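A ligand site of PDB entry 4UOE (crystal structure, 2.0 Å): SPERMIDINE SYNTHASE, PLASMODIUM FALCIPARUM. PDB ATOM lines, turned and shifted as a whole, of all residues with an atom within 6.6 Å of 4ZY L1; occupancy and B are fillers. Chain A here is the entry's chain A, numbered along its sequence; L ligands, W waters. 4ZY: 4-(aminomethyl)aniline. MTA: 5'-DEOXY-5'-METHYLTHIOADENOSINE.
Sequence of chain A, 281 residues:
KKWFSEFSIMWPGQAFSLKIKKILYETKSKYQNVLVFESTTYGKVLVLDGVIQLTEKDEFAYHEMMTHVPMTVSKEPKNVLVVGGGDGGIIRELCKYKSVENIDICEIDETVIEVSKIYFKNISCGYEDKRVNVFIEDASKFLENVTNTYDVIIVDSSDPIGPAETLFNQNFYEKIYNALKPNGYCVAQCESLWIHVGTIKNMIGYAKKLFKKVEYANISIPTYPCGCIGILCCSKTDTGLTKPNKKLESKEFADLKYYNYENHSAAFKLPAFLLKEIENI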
ATOM      1  N   GLU A   6       0.762  18.490  -5.701  1.00  0.00           N
ATOM      2  CA  GLU A   6       2.020  18.000  -6.227  1.00  0.00           C
ATOM      3  C   GLU A   6       2.303  16.503  -5.997  1.00  0.00           C
ATOM      4  O   GLU A   6       2.909  16.110  -4.992  1.00  0.00           O
ATOM      5  CB  GLU A   6       3.138  18.863  -5.590  1.00  0.00           C
ATOM      6  CG  GLU A   6       4.524  18.657  -6.198  1.00  0.00           C
ATOM      7  CD  GLU A   6       5.624  19.314  -5.354  1.00  0.00           C
ATOM      8  OE1 GLU A   6       5.695  19.052  -4.120  1.00  0.00           O
ATOM      9  OE2 GLU A   6       6.434  20.103  -5.922  1.00  0.00           O
ATOM     10  N   MET A  10       8.592  10.513  -7.790  1.00  0.00           N
ATOM     11  CA  MET A  10       9.778  10.821  -6.999  1.00  0.00           C
ATOM     12  C   MET A  10       9.496  10.961  -5.491  1.00  0.00           C
ATOM     13  O   MET A  10      10.398  10.987  -4.674  1.00  0.00           O
ATOM     14  CB  MET A  10      10.400  12.099  -7.546  1.00  0.00           C
ATOM     15  CG  MET A  10      10.787  11.960  -9.056  1.00  0.00           C
ATOM     16  SD  MET A  10      11.491  13.478  -9.709  1.00  0.00           S
ATOM     17  CE  MET A  10      10.150  14.679  -9.639  1.00  0.00           C
ATOM     18  N   TRP A  11       8.234  11.094  -5.109  1.00  0.00           N
ATOM     19  CA  TRP A  11       7.862  11.053  -3.669  1.00  0.00           C
ATOM     20  C   TRP A  11       6.493  10.362  -3.548  1.00  0.00           C
ATOM     21  O   TRP A  11       5.427  11.006  -3.274  1.00  0.00           O
ATOM     22  CB  TRP A  11       7.824  12.464  -3.050  1.00  0.00           C
ATOM     23  CG  TRP A  11       7.334  13.577  -3.913  1.00  0.00           C
ATOM     24  CD1 TRP A  11       6.079  14.033  -4.027  1.00  0.00           C
ATOM     25  CD2 TRP A  11       8.142  14.417  -4.753  1.00  0.00           C
ATOM     26  NE1 TRP A  11       6.021  15.111  -4.901  1.00  0.00           N
ATOM     27  CE2 TRP A  11       7.285  15.361  -5.353  1.00  0.00           C
ATOM     28  CE3 TRP A  11       9.509  14.460  -5.048  1.00  0.00           C
ATOM     29  CZ2 TRP A  11       7.740  16.324  -6.265  1.00  0.00           C
ATOM     30  CZ3 TRP A  11       9.954  15.402  -5.953  1.00  0.00           C
ATOM     31  CH2 TRP A  11       9.070  16.341  -6.545  1.00  0.00           C
ATOM     32  N   VAL A  51       5.648  19.941 -10.889  1.00  0.00           N
ATOM     33  CA  VAL A  51       6.495  20.032  -9.685  1.00  0.00           C
ATOM     34  C   VAL A  51       6.792  21.482  -9.333  1.00  0.00           C
ATOM     35  O   VAL A  51       7.223  22.252 -10.188  1.00  0.00           O
ATOM     36  CB  VAL A  51       7.809  19.336  -9.876  1.00  0.00           C
ATOM     37  CG1 VAL A  51       8.697  19.541  -8.652  1.00  0.00           C
ATOM     38  CG2 VAL A  51       7.585  17.844 -10.190  1.00  0.00           C
ATOM     39  N   ILE A  52       6.591  21.845  -8.078  1.00  0.00           N
ATOM     40  CA  ILE A  52       6.692  23.230  -7.668  1.00  0.00           C
ATOM     41  C   ILE A  52       8.132  23.639  -7.692  1.00  0.00           C
ATOM     42  O   ILE A  52       8.970  22.921  -7.149  1.00  0.00           O
ATOM     43  CB  ILE A  52       6.178  23.448  -6.225  1.00  0.00           C
ATOM     44  CG1 ILE A  52       4.689  23.188  -6.160  1.00  0.00           C
ATOM     45  CG2 ILE A  52       6.555  24.844  -5.774  1.00  0.00           C
ATOM     46  CD1 ILE A  52       4.093  23.099  -4.733  1.00  0.00           C
ATOM     47  N   GLN A  53       8.431  24.778  -8.327  1.00  0.00           N
ATOM     48  CA  GLN A  53       9.822  25.229  -8.433  1.00  0.00           C
ATOM     49  C   GLN A  53      10.078  26.368  -7.502  1.00  0.00           C
ATOM     50  O   GLN A  53      11.155  26.500  -6.967  1.00  0.00           O
ATOM     51  CB  GLN A  53      10.174  25.678  -9.866  1.00  0.00           C
ATOM     52  CG  GLN A  53       9.830  24.661 -10.912  1.00  0.00           C
ATOM     53  CD  GLN A  53      10.757  23.452 -10.937  1.00  0.00           C
ATOM     54  OE1 GLN A  53      10.300  22.286 -10.948  1.00  0.00           O
ATOM     55  NE2 GLN A  53      12.040  23.717 -11.030  1.00  0.00           N
ATOM     56  N   LEU A  54       9.105  27.227  -7.316  1.00  0.00           N
ATOM     57  CA  LEU A  54       9.233  28.227  -6.292  1.00  0.00           C
ATOM     58  C   LEU A  54       7.915  28.788  -5.933  1.00  0.00           C
ATOM     59  O   LEU A  54       6.963  28.607  -6.661  1.00  0.00           O
ATOM     60  CB  LEU A  54      10.158  29.363  -6.748  1.00  0.00           C
ATOM     61  CG  LEU A  54       9.762  30.247  -7.965  1.00  0.00           C
ATOM     62  CD1 LEU A  54       8.809  31.402  -7.659  1.00  0.00           C
ATOM     63  CD2 LEU A  54      11.047  30.793  -8.566  1.00  0.00           C
ATOM     64  N   TYR A  62      15.846  29.292  -0.264  1.00  0.00           N
ATOM     65  CA  TYR A  62      16.673  28.440  -1.179  1.00  0.00           C
ATOM     66  C   TYR A  62      17.663  29.285  -2.037  1.00  0.00           C
ATOM     67  O   TYR A  62      18.812  28.902  -2.249  1.00  0.00           O
ATOM     68  CB  TYR A  62      15.783  27.625  -2.081  1.00  0.00           C
ATOM     69  CG  TYR A  62      16.497  26.879  -3.213  1.00  0.00           C
ATOM     70  CD1 TYR A  62      17.189  25.745  -2.978  1.00  0.00           C
ATOM     71  CD2 TYR A  62      16.404  27.313  -4.516  1.00  0.00           C
ATOM     72  CE1 TYR A  62      17.803  25.017  -4.038  1.00  0.00           C
ATOM     73  CE2 TYR A  62      17.041  26.631  -5.576  1.00  0.00           C
ATOM     74  CZ  TYR A  62      17.728  25.497  -5.332  1.00  0.00           C
ATOM     75  OH  TYR A  62      18.336  24.818  -6.406  1.00  0.00           O
ATOM     76  N   HIS A  63      17.209  30.418  -2.532  1.00  0.00           N
ATOM     77  CA  HIS A  63      18.072  31.305  -3.322  1.00  0.00           C
ATOM     78  C   HIS A  63      19.226  31.949  -2.506  1.00  0.00           C
ATOM     79  O   HIS A  63      20.378  31.859  -2.944  1.00  0.00           O
ATOM     80  CB  HIS A  63      17.229  32.317  -4.074  1.00  0.00           C
ATOM     81  CG  HIS A  63      16.354  31.673  -5.117  1.00  0.00           C
ATOM     82  ND1 HIS A  63      15.035  32.023  -5.319  1.00  0.00           N
ATOM     83  CD2 HIS A  63      16.621  30.660  -5.982  1.00  0.00           C
ATOM     84  CE1 HIS A  63      14.539  31.273  -6.278  1.00  0.00           C
ATOM     85  NE2 HIS A  63      15.491  30.453  -6.711  1.00  0.00           N
ATOM     86  N   GLY A  85      18.063  27.633 -13.177  1.00  0.00           N
ATOM     87  CA  GLY A  85      17.802  28.931 -12.605  1.00  0.00           C
ATOM     88  C   GLY A  85      17.125  30.018 -13.451  1.00  0.00           C
ATOM     89  O   GLY A  85      17.317  31.226 -13.128  1.00  0.00           O
ATOM     90  N   ASP A  87      14.351  31.238 -13.392  1.00  0.00           N
ATOM     91  CA  ASP A  87      13.572  32.255 -12.634  1.00  0.00           C
ATOM     92  C   ASP A  87      14.394  33.487 -12.357  1.00  0.00           C
ATOM     93  O   ASP A  87      13.849  34.591 -12.144  1.00  0.00           O
ATOM     94  CB  ASP A  87      13.054  31.685 -11.331  1.00  0.00           C
ATOM     95  CG  ASP A  87      14.104  30.954 -10.566  1.00  0.00           C
ATOM     96  OD1 ASP A  87      14.333  29.745 -10.851  1.00  0.00           O
ATOM     97  OD2 ASP A  87      14.738  31.615  -9.738  1.00  0.00           O
ATOM     98  N   ASP A 156      21.279  25.211 -10.168  1.00  0.00           N
ATOM     99  CA  ASP A 156      19.912  25.367  -9.751  1.00  0.00           C
ATOM    100  C   ASP A 156      18.991  24.618 -10.738  1.00  0.00           C
ATOM    101  O   ASP A 156      18.257  25.210 -11.485  1.00  0.00           O
ATOM    102  CB  ASP A 156      19.537  26.823  -9.645  1.00  0.00           C
ATOM    103  CG  ASP A 156      18.121  27.019  -9.244  1.00  0.00           C
ATOM    104  OD1 ASP A 156      17.454  26.028  -8.892  1.00  0.00           O
ATOM    105  OD2 ASP A 156      17.658  28.148  -9.315  1.00  0.00           O
ATOM    106  N   SER A 157      19.053  23.288 -10.704  1.00  0.00           N
ATOM    107  CA  SER A 157      18.232  22.452 -11.549  1.00  0.00           C
ATOM    108  C   SER A 157      16.847  22.098 -10.989  1.00  0.00           C
ATOM    109  O   SER A 157      16.554  22.186  -9.813  1.00  0.00           O
ATOM    110  CB  SER A 157      18.925  21.137 -11.806  1.00  0.00           C
ATOM    111  OG  SER A 157      18.890  20.309 -10.656  1.00  0.00           O
ATOM    112  N   SER A 158      16.021  21.684 -11.908  1.00  0.00           N
ATOM    113  CA  SER A 158      14.819  20.938 -11.589  1.00  0.00           C
ATOM    114  C   SER A 158      15.253  19.463 -11.258  1.00  0.00           C
ATOM    115  O   SER A 158      16.451  19.126 -11.344  1.00  0.00           O
ATOM    116  CB  SER A 158      13.845  21.016 -12.792  1.00  0.00           C
ATOM    117  OG  SER A 158      14.567  20.715 -13.992  1.00  0.00           O
ATOM    118  N   ASP A 159      14.272  18.619 -10.936  1.00  0.00           N
ATOM    119  CA  ASP A 159      14.475  17.240 -10.523  1.00  0.00           C
ATOM    120  C   ASP A 159      14.849  16.326 -11.694  1.00  0.00           C
ATOM    121  O   ASP A 159      14.653  16.684 -12.846  1.00  0.00           O
ATOM    122  CB  ASP A 159      13.184  16.724  -9.835  1.00  0.00           C
ATOM    123  CG  ASP A 159      12.764  17.551  -8.620  1.00  0.00           C
ATOM    124  OD1 ASP A 159      13.553  17.725  -7.661  1.00  0.00           O
ATOM    125  OD2 ASP A 159      11.633  18.047  -8.614  1.00  0.00           O
ATOM    126  N   GLN A 189      21.617  21.578  -6.261  1.00  0.00           N
ATOM    127  CA  GLN A 189      20.375  21.129  -5.615  1.00  0.00           C
ATOM    128  C   GLN A 189      20.511  19.614  -5.540  1.00  0.00           C
ATOM    129  O   GLN A 189      20.902  18.928  -6.547  1.00  0.00           O
ATOM    130  CB  GLN A 189      19.191  21.560  -6.504  1.00  0.00           C
ATOM    131  CG  GLN A 189      17.786  21.152  -6.101  1.00  0.00           C
ATOM    132  CD  GLN A 189      17.435  19.744  -6.527  1.00  0.00           C
ATOM    133  OE1 GLN A 189      17.410  18.868  -5.709  1.00  0.00           O
ATOM    134  NE2 GLN A 189      17.127  19.540  -7.799  1.00  0.00           N
ATOM    135  N   GLU A 191      18.329  17.570  -3.338  1.00  0.00           N
ATOM    136  CA  GLU A 191      17.142  16.841  -2.988  1.00  0.00           C
ATOM    137  C   GLU A 191      16.995  16.746  -1.442  1.00  0.00           C
ATOM    138  O   GLU A 191      17.641  17.523  -0.698  1.00  0.00           O
ATOM    139  CB  GLU A 191      17.137  15.459  -3.719  1.00  0.00           C
ATOM    140  CG  GLU A 191      17.061  15.549  -5.258  1.00  0.00           C
ATOM    141  CD  GLU A 191      15.740  16.109  -5.858  1.00  0.00           C
ATOM    142  OE1 GLU A 191      14.729  16.419  -5.112  1.00  0.00           O
ATOM    143  OE2 GLU A 191      15.683  16.215  -7.127  1.00  0.00           O
ATOM    144  N   THR A 223       7.964  24.505   0.647  1.00  0.00           N
ATOM    145  CA  THR A 223       7.293  24.157  -0.609  1.00  0.00           C
ATOM    146  C   THR A 223       8.065  23.238  -1.472  1.00  0.00           C
ATOM    147  O   THR A 223       7.693  23.017  -2.609  1.00  0.00           O
ATOM    148  CB  THR A 223       6.805  25.391  -1.404  1.00  0.00           C
ATOM    149  OG1 THR A 223       7.895  26.260  -1.705  1.00  0.00           O
ATOM    150  CG2 THR A 223       5.765  26.196  -0.589  1.00  0.00           C
ATOM    151  N   TYR A 224       9.142  22.669  -0.954  1.00  0.00           N
ATOM    152  CA  TYR A 224       9.674  21.471  -1.589  1.00  0.00           C
ATOM    153  C   TYR A 224       9.235  20.284  -0.768  1.00  0.00           C
ATOM    154  O   TYR A 224       8.856  20.427   0.408  1.00  0.00           O
ATOM    155  CB  TYR A 224      11.187  21.493  -1.797  1.00  0.00           C
ATOM    156  CG  TYR A 224      11.696  22.567  -2.738  1.00  0.00           C
ATOM    157  CD1 TYR A 224      11.013  22.896  -3.895  1.00  0.00           C
ATOM    158  CD2 TYR A 224      12.859  23.275  -2.447  1.00  0.00           C
ATOM    159  CE1 TYR A 224      11.479  23.891  -4.734  1.00  0.00           C
ATOM    160  CE2 TYR A 224      13.334  24.250  -3.292  1.00  0.00           C
ATOM    161  CZ  TYR A 224      12.648  24.569  -4.439  1.00  0.00           C
ATOM    162  OH  TYR A 224      13.104  25.615  -5.262  1.00  0.00           O
ATOM    163  N   PRO A 225       9.206  19.126  -1.390  1.00  0.00           N
ATOM    164  CA  PRO A 225       8.713  17.954  -0.698  1.00  0.00           C
ATOM    165  C   PRO A 225       9.507  17.619   0.561  1.00  0.00           C
ATOM    166  O   PRO A 225      10.728  17.655   0.551  1.00  0.00           O
ATOM    167  CB  PRO A 225       8.890  16.822  -1.710  1.00  0.00           C
ATOM    168  CG  PRO A 225       9.059  17.451  -3.037  1.00  0.00           C
ATOM    169  CD  PRO A 225       9.533  18.862  -2.806  1.00  0.00           C
ATOM    170  N   ILE A 229      15.468  20.958   1.395  1.00  0.00           N
ATOM    171  CA  ILE A 229      16.242  20.648   0.189  1.00  0.00           C
ATOM    172  C   ILE A 229      17.720  20.674   0.515  1.00  0.00           C
ATOM    173  O   ILE A 229      18.193  21.560   1.179  1.00  0.00           O
ATOM    174  CB  ILE A 229      15.864  21.597  -1.031  1.00  0.00           C
ATOM    175  CG1 ILE A 229      16.349  21.031  -2.328  1.00  0.00           C
ATOM    176  CG2 ILE A 229      16.436  22.997  -0.895  1.00  0.00           C
ATOM    177  CD1 ILE A 229      15.532  19.865  -2.761  1.00  0.00           C
HETATM  178  N1  4ZY L   1      15.209  24.274  -8.741  1.00  0.00           N
HETATM  179  C1  4ZY L   1      14.970  24.030  -7.342  1.00  0.00           C
HETATM  180  C2  4ZY L   1      14.101  22.804  -7.058  1.00  0.00           C
HETATM  181  C7  4ZY L   1      13.085  22.446  -7.953  1.00  0.00           C
HETATM  182  C6  4ZY L   1      12.295  21.323  -7.719  1.00  0.00           C
HETATM  183  C5  4ZY L   1      12.443  20.556  -6.553  1.00  0.00           C
HETATM  184  C4  4ZY L   1      13.437  20.911  -5.637  1.00  0.00           C
HETATM  185  C3  4ZY L   1      14.254  22.039  -5.879  1.00  0.00           C
HETATM  186  N2  4ZY L   1      11.633  19.483  -6.376  1.00  0.00           N
HETATM  187  CS  MTA L   2      13.290  26.616 -12.271  1.00  0.00           C
HETATM  188  S5' MTA L   2      14.942  26.551 -11.719  1.00  0.00           S
HETATM  189  C5' MTA L   2      15.340  24.991 -12.487  1.00  0.00           C
HETATM  190  C4' MTA L   2      15.556  25.126 -13.987  1.00  0.00           C
HETATM  191  O4' MTA L   2      16.321  24.044 -14.481  1.00  0.00           O
HETATM  192  C2' MTA L   2      14.777  24.053 -16.047  1.00  0.00           C
HETATM  193  O2' MTA L   2      14.286  24.362 -17.363  1.00  0.00           O
HETATM  194  C3' MTA L   2      14.359  25.001 -14.944  1.00  0.00           C
HETATM  195  O3' MTA L   2      14.020  26.288 -15.381  1.00  0.00           O
HETATM  196  C1' MTA L   2      16.260  24.079 -15.909  1.00  0.00           C
HETATM  197  N9  MTA L   2      16.882  22.914 -16.510  1.00  0.00           N
HETATM  198  C8  MTA L   2      16.519  21.648 -16.493  1.00  0.00           C
HETATM  199  N7  MTA L   2      17.367  20.845 -17.205  1.00  0.00           N
HETATM  200  C5  MTA L   2      18.335  21.643 -17.636  1.00  0.00           C
HETATM  201  C6  MTA L   2      19.496  21.469 -18.452  1.00  0.00           C
HETATM  202  N6  MTA L   2      19.868  20.233 -18.866  1.00  0.00           N
HETATM  203  N1  MTA L   2      20.224  22.562 -18.660  1.00  0.00           N
HETATM  204  C2  MTA L   2      19.890  23.795 -18.249  1.00  0.00           C
HETATM  205  N3  MTA L   2      18.795  24.024 -17.524  1.00  0.00           N
HETATM  206  C4  MTA L   2      17.993  23.000 -17.208  1.00  0.00           C
HETATM  207  O   HOH W   1      13.317  26.438  -8.775  1.00  0.00           O
HETATM  208  O   HOH W   2       9.126  20.639  -5.502  1.00  0.00           O
HETATM  209  O   HOH W   3      12.673  17.913  -4.345  1.00  0.00           O
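Water W3 lies within hydrogen-bond range of the side-chain carboxylate (OE1) of Glu 191 (2.7 Å), a nitrogen (N2) of 4ZY L1 (2.8 Å) and the side-chain carboxylate (OD1) of Asp 159 (3.4 Å).
Water W1 lies within hydrogen-bond range of the backbone carbonyl oxygen (O) of Gln 53, a nitrogen (N1) of 4ZY L1 and a sulfur (S5') of MTA L2.
Water W2 lies within hydrogen-bond range of OE2 of Glu 6 (2.8 Å), O of Ile 52 (2.8 Å) and N2 of 4ZY L1 (2.9 Å).
S5' of MTA L2 lies close to N1 of 4ZY L1 (3.8 Å).
The side-chain carboxylate of Asp 159 lies within hydrogen-bond range of a nitrogen (N2) of 4ZY L1 (2.7 Å).
The backbone carbonyl oxygen (O) of Ser 157 lies within hydrogen-bond range of a nitrogen (N1) of 4ZY L1 (2.7 Å).
OD1 of Asp 156 is in salt-bridge range of N1 of 4ZY L1 (2.9 Å).
A sulfur (S5') of MTA L2 lies close to the backbone NH (N) of Gly 85 (3.6 Å).
Val 51 touches 4ZY L1 (CG1 to N2, 3.7 Å).
Ile 52 touches 4ZY L1.
NE2 of Gln 53 touches C7 of 4ZY L1 (3.5 Å).
Tyr 62 touches 4ZY L1 (OH to C1, 3.6 Å).
Gln 189 touches 4ZY L1.
OH of Tyr 224 touches C1 of 4ZY L1 (3.2 Å).
CD1 of Ile 229 touches C4 of 4ZY L1, 3.7 Å away.
Hydrophobic or aromatic side chains within 4 Å of 4ZY L1: Val 51, Tyr 62, Tyr 224 and Ile 229.
The nearest printed residue that does not touch 4ZY L1 is Trp 11 (4.1 Å).
OD1 of Asp 159 sits close to OE2 of Glu 191 (2.7 Å).
The backbone carbonyl oxygen (O) of Ser 157 lies within hydrogen-bond range of the side-chain amide nitrogen (NE2) of Gln 189 (3.4 Å).
The side-chain carboxylate of Asp 156 lies within hydrogen-bond range of the side-chain hydroxyl of Tyr 62 (2.9 Å).
O of Asp 156 is in hydrogen-bond range of N of Gly 85, 3.0 Å away.
OH of Tyr 224 is in hydrogen-bond range of O of Gln 53 (2.7 Å).
O of Val 51 lies close to OE1 of Gln 53, 3.2 Å away.
OE1 of Gln 189 is in hydrogen-bond range of N of Glu 191 (2.9 Å).
The side-chain carboxylate (OE2) of Glu 6 sits at hydrogen-bond distance from the backbone NH (N) of Ile 52, at 2.8 Å.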
